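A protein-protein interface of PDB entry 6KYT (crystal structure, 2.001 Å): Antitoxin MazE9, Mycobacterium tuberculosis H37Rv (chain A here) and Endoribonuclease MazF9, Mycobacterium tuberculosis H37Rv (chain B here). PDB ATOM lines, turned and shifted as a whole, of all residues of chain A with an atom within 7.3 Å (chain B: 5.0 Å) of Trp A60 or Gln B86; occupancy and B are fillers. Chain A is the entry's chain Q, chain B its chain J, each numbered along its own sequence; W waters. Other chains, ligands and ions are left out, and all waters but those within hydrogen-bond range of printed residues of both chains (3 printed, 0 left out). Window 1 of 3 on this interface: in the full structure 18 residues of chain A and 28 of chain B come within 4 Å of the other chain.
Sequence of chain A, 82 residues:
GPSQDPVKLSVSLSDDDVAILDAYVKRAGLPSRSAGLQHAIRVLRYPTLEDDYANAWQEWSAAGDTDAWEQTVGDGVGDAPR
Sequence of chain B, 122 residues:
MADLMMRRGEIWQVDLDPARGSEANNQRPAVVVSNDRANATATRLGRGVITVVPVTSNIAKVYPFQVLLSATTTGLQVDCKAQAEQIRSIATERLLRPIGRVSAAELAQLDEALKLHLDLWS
Among the printed residues, pairs that only touch across the chains: Trp A69 with Pro B54 (3.7 Å), Trp A69 with Arg B88 (3.8 Å), Trp A60 with Gln B83 (3.8 Å), Trp A60 with Pro B54 (3.9 Å), Trp A60 with Arg B88 (3.9 Å) and Ala A56 with Glu B85 (3.9 Å).
The side-chain carboxylate (OE2) of Glu B85 is in hydrogen-bond range of the side-chain amide nitrogen (NE2) of Gln B83 (2.6 Å). The backbone carbonyl oxygen of Trp A60 is in hydrogen-bond range of the side-chain hydroxyl of Thr A66 (2.6 Å). The backbone carbonyl oxygen (O) of Arg B88 is in hydrogen-bond range of the backbone NH (N) of Val B52. The backbone NH (N) of Gln B83 is in hydrogen-bond range of the backbone carbonyl oxygen (O) of Pro B54 (2.9 Å). The side-chain amide oxygen of Gln B83 sits at hydrogen-bond distance from the side-chain hydroxyl of Thr B56 (2.7 Å). The side-chain amide oxygen of Gln B86 lies within hydrogen-bond range of the guanidinium group of Arg B88.
Trp A60 touches just these residues of chain B: Pro B54, Gln B83, Gln B86 and Arg B88. Of the printed residues of chain B, Trp A69 touches Pro B54 and Arg B88. Of the printed residues of chain B, Ala A56 touches Glu B85 (3.9 Å). Of the printed residues of chain A, Gln B83 touches Trp A60. Printed residues of chain A within 4 Å of Glu B85: Ala A56. The nearest residue of chain A that does not touch Gln B86 is Trp A57 (4.2 Å).
Of the 9 printed residues of chain B, 5 touch a printed residue of chain A. Printed residues of chain B that touch a printed residue of chain A: Pro B54, Gln B83, Glu B85, Gln B86 and Arg B88. Along chain B the printed residues that touch a printed residue of chain A span positions 54 to 88. Hydrophobic or aromatic side chains of chain A that line the printed part of chain B: Ala A56, Trp A60 and Trp A69. Among the printed residues, 7 pairs touch across the chains. Among the printed residues, no Asp or Glu carboxylate lies within 4 Å of a Lys or Arg side-chain nitrogen of the other chain.
Water W3 lies within hydrogen-bond range of OE2 of Glu B85 (2.7 Å), NE2 of Gln B86 (2.9 Å), O of Ala A56 (3.1 Å) and NE2 of Gln B83 (3.5 Å). Water W2 lies within hydrogen-bond range of the backbone carbonyl oxygen of Glu B85 and the indole nitrogen of Trp A57. Water W1 lies within hydrogen-bond range of the side-chain amide nitrogen of Gln B83 (3.0 Å) and the backbone carbonyl oxygen of Ala A56 (3.1 Å).
The side-chain amide oxygen (OE1) of Gln B86 lies close to the indole nitrogen (NE1) of Trp A60, 3.5 Å away.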
ATOM      1  N   ALA A  54     -24.635  23.311  33.577  1.00  0.00           N
ATOM      2  CA  ALA A  54     -25.374  24.005  32.524  1.00  0.00           C
ATOM      3  C   ALA A  54     -24.602  23.984  31.209  1.00  0.00           C
ATOM      4  O   ALA A  54     -25.149  23.637  30.151  1.00  0.00           O
ATOM      5  CB  ALA A  54     -25.675  25.440  32.953  1.00  0.00           C
ATOM      6  N   ASN A  55     -23.313  24.326  31.263  1.00  0.00           N
ATOM      7  CA  ASN A  55     -22.508  24.382  30.048  1.00  0.00           C
ATOM      8  C   ASN A  55     -22.263  22.993  29.471  1.00  0.00           C
ATOM      9  O   ASN A  55     -22.324  22.805  28.251  1.00  0.00           O
ATOM     10  CB  ASN A  55     -21.186  25.092  30.335  1.00  0.00           C
ATOM     11  CG  ASN A  55     -21.355  26.587  30.516  1.00  0.00           C
ATOM     12  OD1 ASN A  55     -22.023  27.246  29.720  1.00  0.00           O
ATOM     13  ND2 ASN A  55     -20.757  27.130  31.571  1.00  0.00           N
ATOM     14  N   ALA A  56     -21.982  22.008  30.328  1.00  0.00           N
ATOM     15  CA  ALA A  56     -21.739  20.653  29.838  1.00  0.00           C
ATOM     16  C   ALA A  56     -22.971  20.090  29.143  1.00  0.00           C
ATOM     17  O   ALA A  56     -22.868  19.479  28.071  1.00  0.00           O
ATOM     18  CB  ALA A  56     -21.311  19.747  30.990  1.00  0.00           C
ATOM     19  N   TRP A  57     -24.149  20.290  29.739  1.00  0.00           N
ATOM     20  CA  TRP A  57     -25.387  19.852  29.106  1.00  0.00           C
ATOM     21  C   TRP A  57     -25.626  20.593  27.799  1.00  0.00           C
ATOM     22  O   TRP A  57     -26.106  20.001  26.824  1.00  0.00           O
ATOM     23  CB  TRP A  57     -26.564  20.060  30.056  1.00  0.00           C
ATOM     24  CG  TRP A  57     -26.508  19.218  31.292  1.00  0.00           C
ATOM     25  CD1 TRP A  57     -25.862  18.027  31.447  1.00  0.00           C
ATOM     26  CD2 TRP A  57     -27.118  19.512  32.553  1.00  0.00           C
ATOM     27  NE1 TRP A  57     -26.037  17.557  32.727  1.00  0.00           N
ATOM     28  CE2 TRP A  57     -26.804  18.452  33.426  1.00  0.00           C
ATOM     29  CE3 TRP A  57     -27.900  20.568  33.029  1.00  0.00           C
ATOM     30  CZ2 TRP A  57     -27.245  18.417  34.747  1.00  0.00           C
ATOM     31  CZ3 TRP A  57     -28.337  20.531  34.338  1.00  0.00           C
ATOM     32  CH2 TRP A  57     -28.009  19.465  35.184  1.00  0.00           C
ATOM     33  N   GLN A  58     -25.300  21.889  27.757  1.00  0.00           N
ATOM     34  CA  GLN A  58     -25.518  22.649  26.529  1.00  0.00           C
ATOM     35  C   GLN A  58     -24.614  22.159  25.403  1.00  0.00           C
ATOM     36  O   GLN A  58     -25.056  22.039  24.256  1.00  0.00           O
ATOM     37  CB  GLN A  58     -25.300  24.140  26.779  1.00  0.00           C
ATOM     38  CG  GLN A  58     -25.485  24.999  25.538  1.00  0.00           C
ATOM     39  CD  GLN A  58     -25.467  26.481  25.849  1.00  0.00           C
ATOM     40  OE1 GLN A  58     -24.431  27.137  25.744  1.00  0.00           O
ATOM     41  NE2 GLN A  58     -26.620  27.018  26.232  1.00  0.00           N
ATOM     42  N   GLU A  59     -23.345  21.878  25.707  1.00  0.00           N
ATOM     43  CA  GLU A  59     -22.446  21.339  24.691  1.00  0.00           C
ATOM     44  C   GLU A  59     -22.903  19.955  24.239  1.00  0.00           C
ATOM     45  O   GLU A  59     -22.956  19.668  23.035  1.00  0.00           O
ATOM     46  CB  GLU A  59     -21.017  21.300  25.238  1.00  0.00           C
ATOM     47  CG  GLU A  59     -20.491  22.667  25.701  1.00  0.00           C
ATOM     48  CD  GLU A  59     -19.226  22.578  26.547  1.00  0.00           C
ATOM     49  OE1 GLU A  59     -18.627  21.485  26.631  1.00  0.00           O
ATOM     50  OE2 GLU A  59     -18.830  23.609  27.134  1.00  0.00           O
ATOM     51  N   TRP A  60     -23.263  19.095  25.197  1.00  0.00           N
ATOM     52  CA  TRP A  60     -23.737  17.749  24.887  1.00  0.00           C
ATOM     53  C   TRP A  60     -24.943  17.782  23.955  1.00  0.00           C
ATOM     54  O   TRP A  60     -24.960  17.111  22.916  1.00  0.00           O
ATOM     55  CB  TRP A  60     -24.077  17.020  26.191  1.00  0.00           C
ATOM     56  CG  TRP A  60     -24.692  15.665  26.022  1.00  0.00           C
ATOM     57  CD1 TRP A  60     -26.022  15.361  26.021  1.00  0.00           C
ATOM     58  CD2 TRP A  60     -23.995  14.424  25.858  1.00  0.00           C
ATOM     59  NE1 TRP A  60     -26.198  14.008  25.856  1.00  0.00           N
ATOM     60  CE2 TRP A  60     -24.968  13.410  25.753  1.00  0.00           C
ATOM     61  CE3 TRP A  60     -22.645  14.072  25.784  1.00  0.00           C
ATOM     62  CZ2 TRP A  60     -24.634  12.068  25.578  1.00  0.00           C
ATOM     63  CZ3 TRP A  60     -22.313  12.739  25.609  1.00  0.00           C
ATOM     64  CH2 TRP A  60     -23.304  11.755  25.508  1.00  0.00           C
ATOM     65  N   SER A  61     -25.968  18.562  24.311  1.00  0.00           N
ATOM     66  CA  SER A  61     -27.149  18.661  23.459  1.00  0.00           C
ATOM     67  C   SER A  61     -26.830  19.337  22.134  1.00  0.00           C
ATOM     68  O   SER A  61     -27.443  19.012  21.111  1.00  0.00           O
ATOM     69  CB  SER A  61     -28.262  19.420  24.181  1.00  0.00           C
ATOM     70  OG  SER A  61     -27.886  20.765  24.421  1.00  0.00           O
ATOM     71  N   ALA A  62     -25.880  20.273  22.130  1.00  0.00           N
ATOM     72  CA  ALA A  62     -25.536  20.974  20.898  1.00  0.00           C
ATOM     73  C   ALA A  62     -24.834  20.059  19.903  1.00  0.00           C
ATOM     74  O   ALA A  62     -24.973  20.250  18.689  1.00  0.00           O
ATOM     75  CB  ALA A  62     -24.672  22.194  21.213  1.00  0.00           C
ATOM     76  N   ALA A  63     -24.085  19.069  20.384  1.00  0.00           N
ATOM     77  CA  ALA A  63     -23.430  18.127  19.485  1.00  0.00           C
ATOM     78  C   ALA A  63     -24.447  17.139  18.929  1.00  0.00           C
ATOM     79  O   ALA A  63     -25.212  16.528  19.682  1.00  0.00           O
ATOM     80  CB  ALA A  63     -22.305  17.381  20.204  1.00  0.00           C
ATOM     81  N   GLY A  64     -24.461  16.992  17.602  1.00  0.00           N
ATOM     82  CA  GLY A  64     -25.329  16.015  16.972  1.00  0.00           C
ATOM     83  C   GLY A  64     -24.843  14.586  17.102  1.00  0.00           C
ATOM     84  O   GLY A  64     -25.634  13.656  16.921  1.00  0.00           O
ATOM     85  N   ASP A  65     -23.563  14.391  17.418  1.00  0.00           N
ATOM     86  CA  ASP A  65     -23.003  13.053  17.567  1.00  0.00           C
ATOM     87  C   ASP A  65     -23.330  12.410  18.908  1.00  0.00           C
ATOM     88  O   ASP A  65     -22.877  11.288  19.163  1.00  0.00           O
ATOM     89  CB  ASP A  65     -21.482  13.087  17.364  1.00  0.00           C
ATOM     90  CG  ASP A  65     -20.783  14.087  18.274  1.00  0.00           C
ATOM     91  OD1 ASP A  65     -19.680  14.544  17.909  1.00  0.00           O
ATOM     92  OD2 ASP A  65     -21.325  14.420  19.347  1.00  0.00           O
ATOM     93  N   THR A  66     -24.095  13.083  19.769  1.00  0.00           N
ATOM     94  CA  THR A  66     -24.443  12.537  21.073  1.00  0.00           C
ATOM     95  C   THR A  66     -25.882  12.046  21.161  1.00  0.00           C
ATOM     96  O   THR A  66     -26.173  11.189  22.005  1.00  0.00           O
ATOM     97  CB  THR A  66     -24.201  13.583  22.169  1.00  0.00           C
ATOM     98  OG1 THR A  66     -24.980  14.756  21.895  1.00  0.00           O
ATOM     99  CG2 THR A  66     -22.727  13.957  22.227  1.00  0.00           C
ATOM    100  N   ASP A  67     -26.777  12.555  20.308  1.00  0.00           N
ATOM    101  CA  ASP A  67     -28.176  12.135  20.348  1.00  0.00           C
ATOM    102  C   ASP A  67     -28.319  10.627  20.192  1.00  0.00           C
ATOM    103  O   ASP A  67     -29.268  10.035  20.723  1.00  0.00           O
ATOM    104  CB  ASP A  67     -28.975  12.855  19.261  1.00  0.00           C
ATOM    105  CG  ASP A  67     -28.930  14.364  19.404  1.00  0.00           C
ATOM    106  OD1 ASP A  67     -29.216  15.066  18.411  1.00  0.00           O
ATOM    107  OD2 ASP A  67     -28.606  14.850  20.508  1.00  0.00           O
ATOM    108  N   ALA A  68     -27.384   9.991  19.480  1.00  0.00           N
ATOM    109  CA  ALA A  68     -27.436   8.544  19.296  1.00  0.00           C
ATOM    110  C   ALA A  68     -27.513   7.806  20.627  1.00  0.00           C
ATOM    111  O   ALA A  68     -28.149   6.748  20.713  1.00  0.00           O
ATOM    112  CB  ALA A  68     -26.218   8.077  18.499  1.00  0.00           C
ATOM    113  N   TRP A  69     -26.898   8.360  21.677  1.00  0.00           N
ATOM    114  CA  TRP A  69     -26.899   7.685  22.971  1.00  0.00           C
ATOM    115  C   TRP A  69     -28.310   7.480  23.502  1.00  0.00           C
ATOM    116  O   TRP A  69     -28.564   6.502  24.219  1.00  0.00           O
ATOM    117  CB  TRP A  69     -26.058   8.472  23.975  1.00  0.00           C
ATOM    118  CG  TRP A  69     -24.601   8.216  23.811  1.00  0.00           C
ATOM    119  CD1 TRP A  69     -23.697   8.995  23.151  1.00  0.00           C
ATOM    120  CD2 TRP A  69     -23.877   7.078  24.292  1.00  0.00           C
ATOM    121  NE1 TRP A  69     -22.450   8.419  23.204  1.00  0.00           N
ATOM    122  CE2 TRP A  69     -22.535   7.240  23.898  1.00  0.00           C
ATOM    123  CE3 TRP A  69     -24.234   5.941  25.022  1.00  0.00           C
ATOM    124  CZ2 TRP A  69     -21.548   6.308  24.211  1.00  0.00           C
ATOM    125  CZ3 TRP A  69     -23.253   5.016  25.332  1.00  0.00           C
ATOM    126  CH2 TRP A  69     -21.926   5.206  24.928  1.00  0.00           C
ATOM    127  N   GLU A  70     -29.242   8.369  23.142  1.00  0.00           N
ATOM    128  CA  GLU A  70     -30.626   8.204  23.577  1.00  0.00           C
ATOM    129  C   GLU A  70     -31.161   6.824  23.219  1.00  0.00           C
ATOM    130  O   GLU A  70     -31.954   6.253  23.976  1.00  0.00           O
ATOM    131  CB  GLU A  70     -31.505   9.298  22.967  1.00  0.00           C
ATOM    132  CG  GLU A  70     -32.991   9.196  23.302  1.00  0.00           C
ATOM    133  CD  GLU A  70     -33.739  10.491  23.023  1.00  0.00           C
ATOM    134  OE1 GLU A  70     -34.509  10.940  23.899  1.00  0.00           O
ATOM    135  OE2 GLU A  70     -33.544  11.072  21.934  1.00  0.00           O
ATOM    136  N   VAL B  52     -21.272   2.294  31.263  1.00  0.00           N
ATOM    137  CA  VAL B  52     -20.197   2.983  30.566  1.00  0.00           C
ATOM    138  C   VAL B  52     -20.375   4.488  30.724  1.00  0.00           C
ATOM    139  O   VAL B  52     -21.444   4.986  31.090  1.00  0.00           O
ATOM    140  CB  VAL B  52     -20.139   2.616  29.065  1.00  0.00           C
ATOM    141  CG1 VAL B  52     -20.021   1.111  28.881  1.00  0.00           C
ATOM    142  CG2 VAL B  52     -21.360   3.159  28.338  1.00  0.00           C
ATOM    143  N   PRO B  54     -19.780   7.832  28.363  1.00  0.00           N
ATOM    144  CA  PRO B  54     -19.507   8.238  26.979  1.00  0.00           C
ATOM    145  C   PRO B  54     -18.258   9.101  26.870  1.00  0.00           C
ATOM    146  O   PRO B  54     -17.915   9.864  27.778  1.00  0.00           O
ATOM    147  CB  PRO B  54     -20.763   9.022  26.586  1.00  0.00           C
ATOM    148  CG  PRO B  54     -21.835   8.487  27.485  1.00  0.00           C
ATOM    149  CD  PRO B  54     -21.148   8.171  28.783  1.00  0.00           C
ATOM    150  N   THR B  56     -16.157  11.847  24.320  1.00  0.00           N
ATOM    151  CA  THR B  56     -16.281  12.784  23.211  1.00  0.00           C
ATOM    152  C   THR B  56     -14.942  13.460  22.958  1.00  0.00           C
ATOM    153  O   THR B  56     -14.078  13.521  23.835  1.00  0.00           O
ATOM    154  CB  THR B  56     -17.355  13.857  23.465  1.00  0.00           C
ATOM    155  OG1 THR B  56     -16.953  14.694  24.557  1.00  0.00           O
ATOM    156  CG2 THR B  56     -18.704  13.219  23.779  1.00  0.00           C
ATOM    157  N   GLN B  83     -17.286  11.686  29.974  1.00  0.00           N
ATOM    158  CA  GLN B  83     -18.313  12.540  30.558  1.00  0.00           C
ATOM    159  C   GLN B  83     -19.118  11.702  31.549  1.00  0.00           C
ATOM    160  O   GLN B  83     -20.111  11.067  31.188  1.00  0.00           O
ATOM    161  CB  GLN B  83     -19.187  13.141  29.466  1.00  0.00           C
ATOM    162  CG  GLN B  83     -18.374  13.794  28.356  1.00  0.00           C
ATOM    163  CD  GLN B  83     -19.143  14.863  27.611  1.00  0.00           C
ATOM    164  OE1 GLN B  83     -18.856  15.156  26.451  1.00  0.00           O
ATOM    165  NE2 GLN B  83     -20.126  15.457  28.277  1.00  0.00           N
ATOM    166  N   ALA B  84     -18.672  11.704  32.809  1.00  0.00           N
ATOM    167  CA  ALA B  84     -19.331  10.912  33.841  1.00  0.00           C
ATOM    168  C   ALA B  84     -20.761  11.365  34.097  1.00  0.00           C
ATOM    169  O   ALA B  84     -21.572  10.571  34.587  1.00  0.00           O
ATOM    170  CB  ALA B  84     -18.528  10.968  35.142  1.00  0.00           C
ATOM    171  N   GLU B  85     -21.093  12.617  33.776  1.00  0.00           N
ATOM    172  CA  GLU B  85     -22.467  13.080  33.919  1.00  0.00           C
ATOM    173  C   GLU B  85     -23.404  12.461  32.892  1.00  0.00           C
ATOM    174  O   GLU B  85     -24.614  12.703  32.962  1.00  0.00           O
ATOM    175  CB  GLU B  85     -22.529  14.608  33.821  1.00  0.00           C
ATOM    176  CG  GLU B  85     -22.497  15.170  32.400  1.00  0.00           C
ATOM    177  CD  GLU B  85     -21.106  15.195  31.788  1.00  0.00           C
ATOM    178  OE1 GLU B  85     -20.180  14.584  32.360  1.00  0.00           O
ATOM    179  OE2 GLU B  85     -20.938  15.839  30.730  1.00  0.00           O
ATOM    180  N   GLN B  86     -22.880  11.678  31.946  1.00  0.00           N
ATOM    181  CA  GLN B  86     -23.683  10.985  30.947  1.00  0.00           C
ATOM    182  C   GLN B  86     -23.629   9.470  31.117  1.00  0.00           C
ATOM    183  O   GLN B  86     -23.886   8.733  30.161  1.00  0.00           O
ATOM    184  CB  GLN B  86     -23.230  11.377  29.541  1.00  0.00           C
ATOM    185  CG  GLN B  86     -23.434  12.848  29.216  1.00  0.00           C
ATOM    186  CD  GLN B  86     -24.900  13.225  29.130  1.00  0.00           C
ATOM    187  OE1 GLN B  86     -25.759  12.374  28.899  1.00  0.00           O
ATOM    188  NE2 GLN B  86     -25.194  14.507  29.317  1.00  0.00           N
ATOM    189  N   ILE B  87     -23.302   8.999  32.324  1.00  0.00           N
ATOM    190  CA  ILE B  87     -23.167   7.571  32.582  1.00  0.00           C
ATOM    191  C   ILE B  87     -24.441   6.837  32.178  1.00  0.00           C
ATOM    192  O   ILE B  87     -25.558   7.304  32.427  1.00  0.00           O
ATOM    193  CB  ILE B  87     -22.820   7.353  34.066  1.00  0.00           C
ATOM    194  CG1 ILE B  87     -22.678   5.869  34.392  1.00  0.00           C
ATOM    195  CG2 ILE B  87     -23.854   8.016  34.969  1.00  0.00           C
ATOM    196  CD1 ILE B  87     -22.221   5.606  35.815  1.00  0.00           C
ATOM    197  N   ARG B  88     -24.273   5.683  31.529  1.00  0.00           N
ATOM    198  CA  ARG B  88     -25.406   4.923  31.015  1.00  0.00           C
ATOM    199  C   ARG B  88     -25.109   3.435  31.095  1.00  0.00           C
ATOM    200  O   ARG B  88     -23.977   3.006  30.881  1.00  0.00           O
ATOM    201  CB  ARG B  88     -25.723   5.286  29.560  1.00  0.00           C
ATOM    202  CG  ARG B  88     -26.442   6.603  29.358  1.00  0.00           C
ATOM    203  CD  ARG B  88     -26.432   6.982  27.886  1.00  0.00           C
ATOM    204  NE  ARG B  88     -27.368   8.060  27.584  1.00  0.00           N
ATOM    205  CZ  ARG B  88     -27.134   9.344  27.828  1.00  0.00           C
ATOM    206  NH1 ARG B  88     -28.044  10.256  27.518  1.00  0.00           N
ATOM    207  NH2 ARG B  88     -25.990   9.717  28.387  1.00  0.00           N
HETATM  208  O   HOH W   1     -20.059  18.345  27.378  1.00  0.00           O
HETATM  209  O   HOH W   2     -25.761  15.040  34.080  1.00  0.00           O
HETATM  210  O   HOH W   3     -23.191  16.649  29.394  1.00  0.00           O
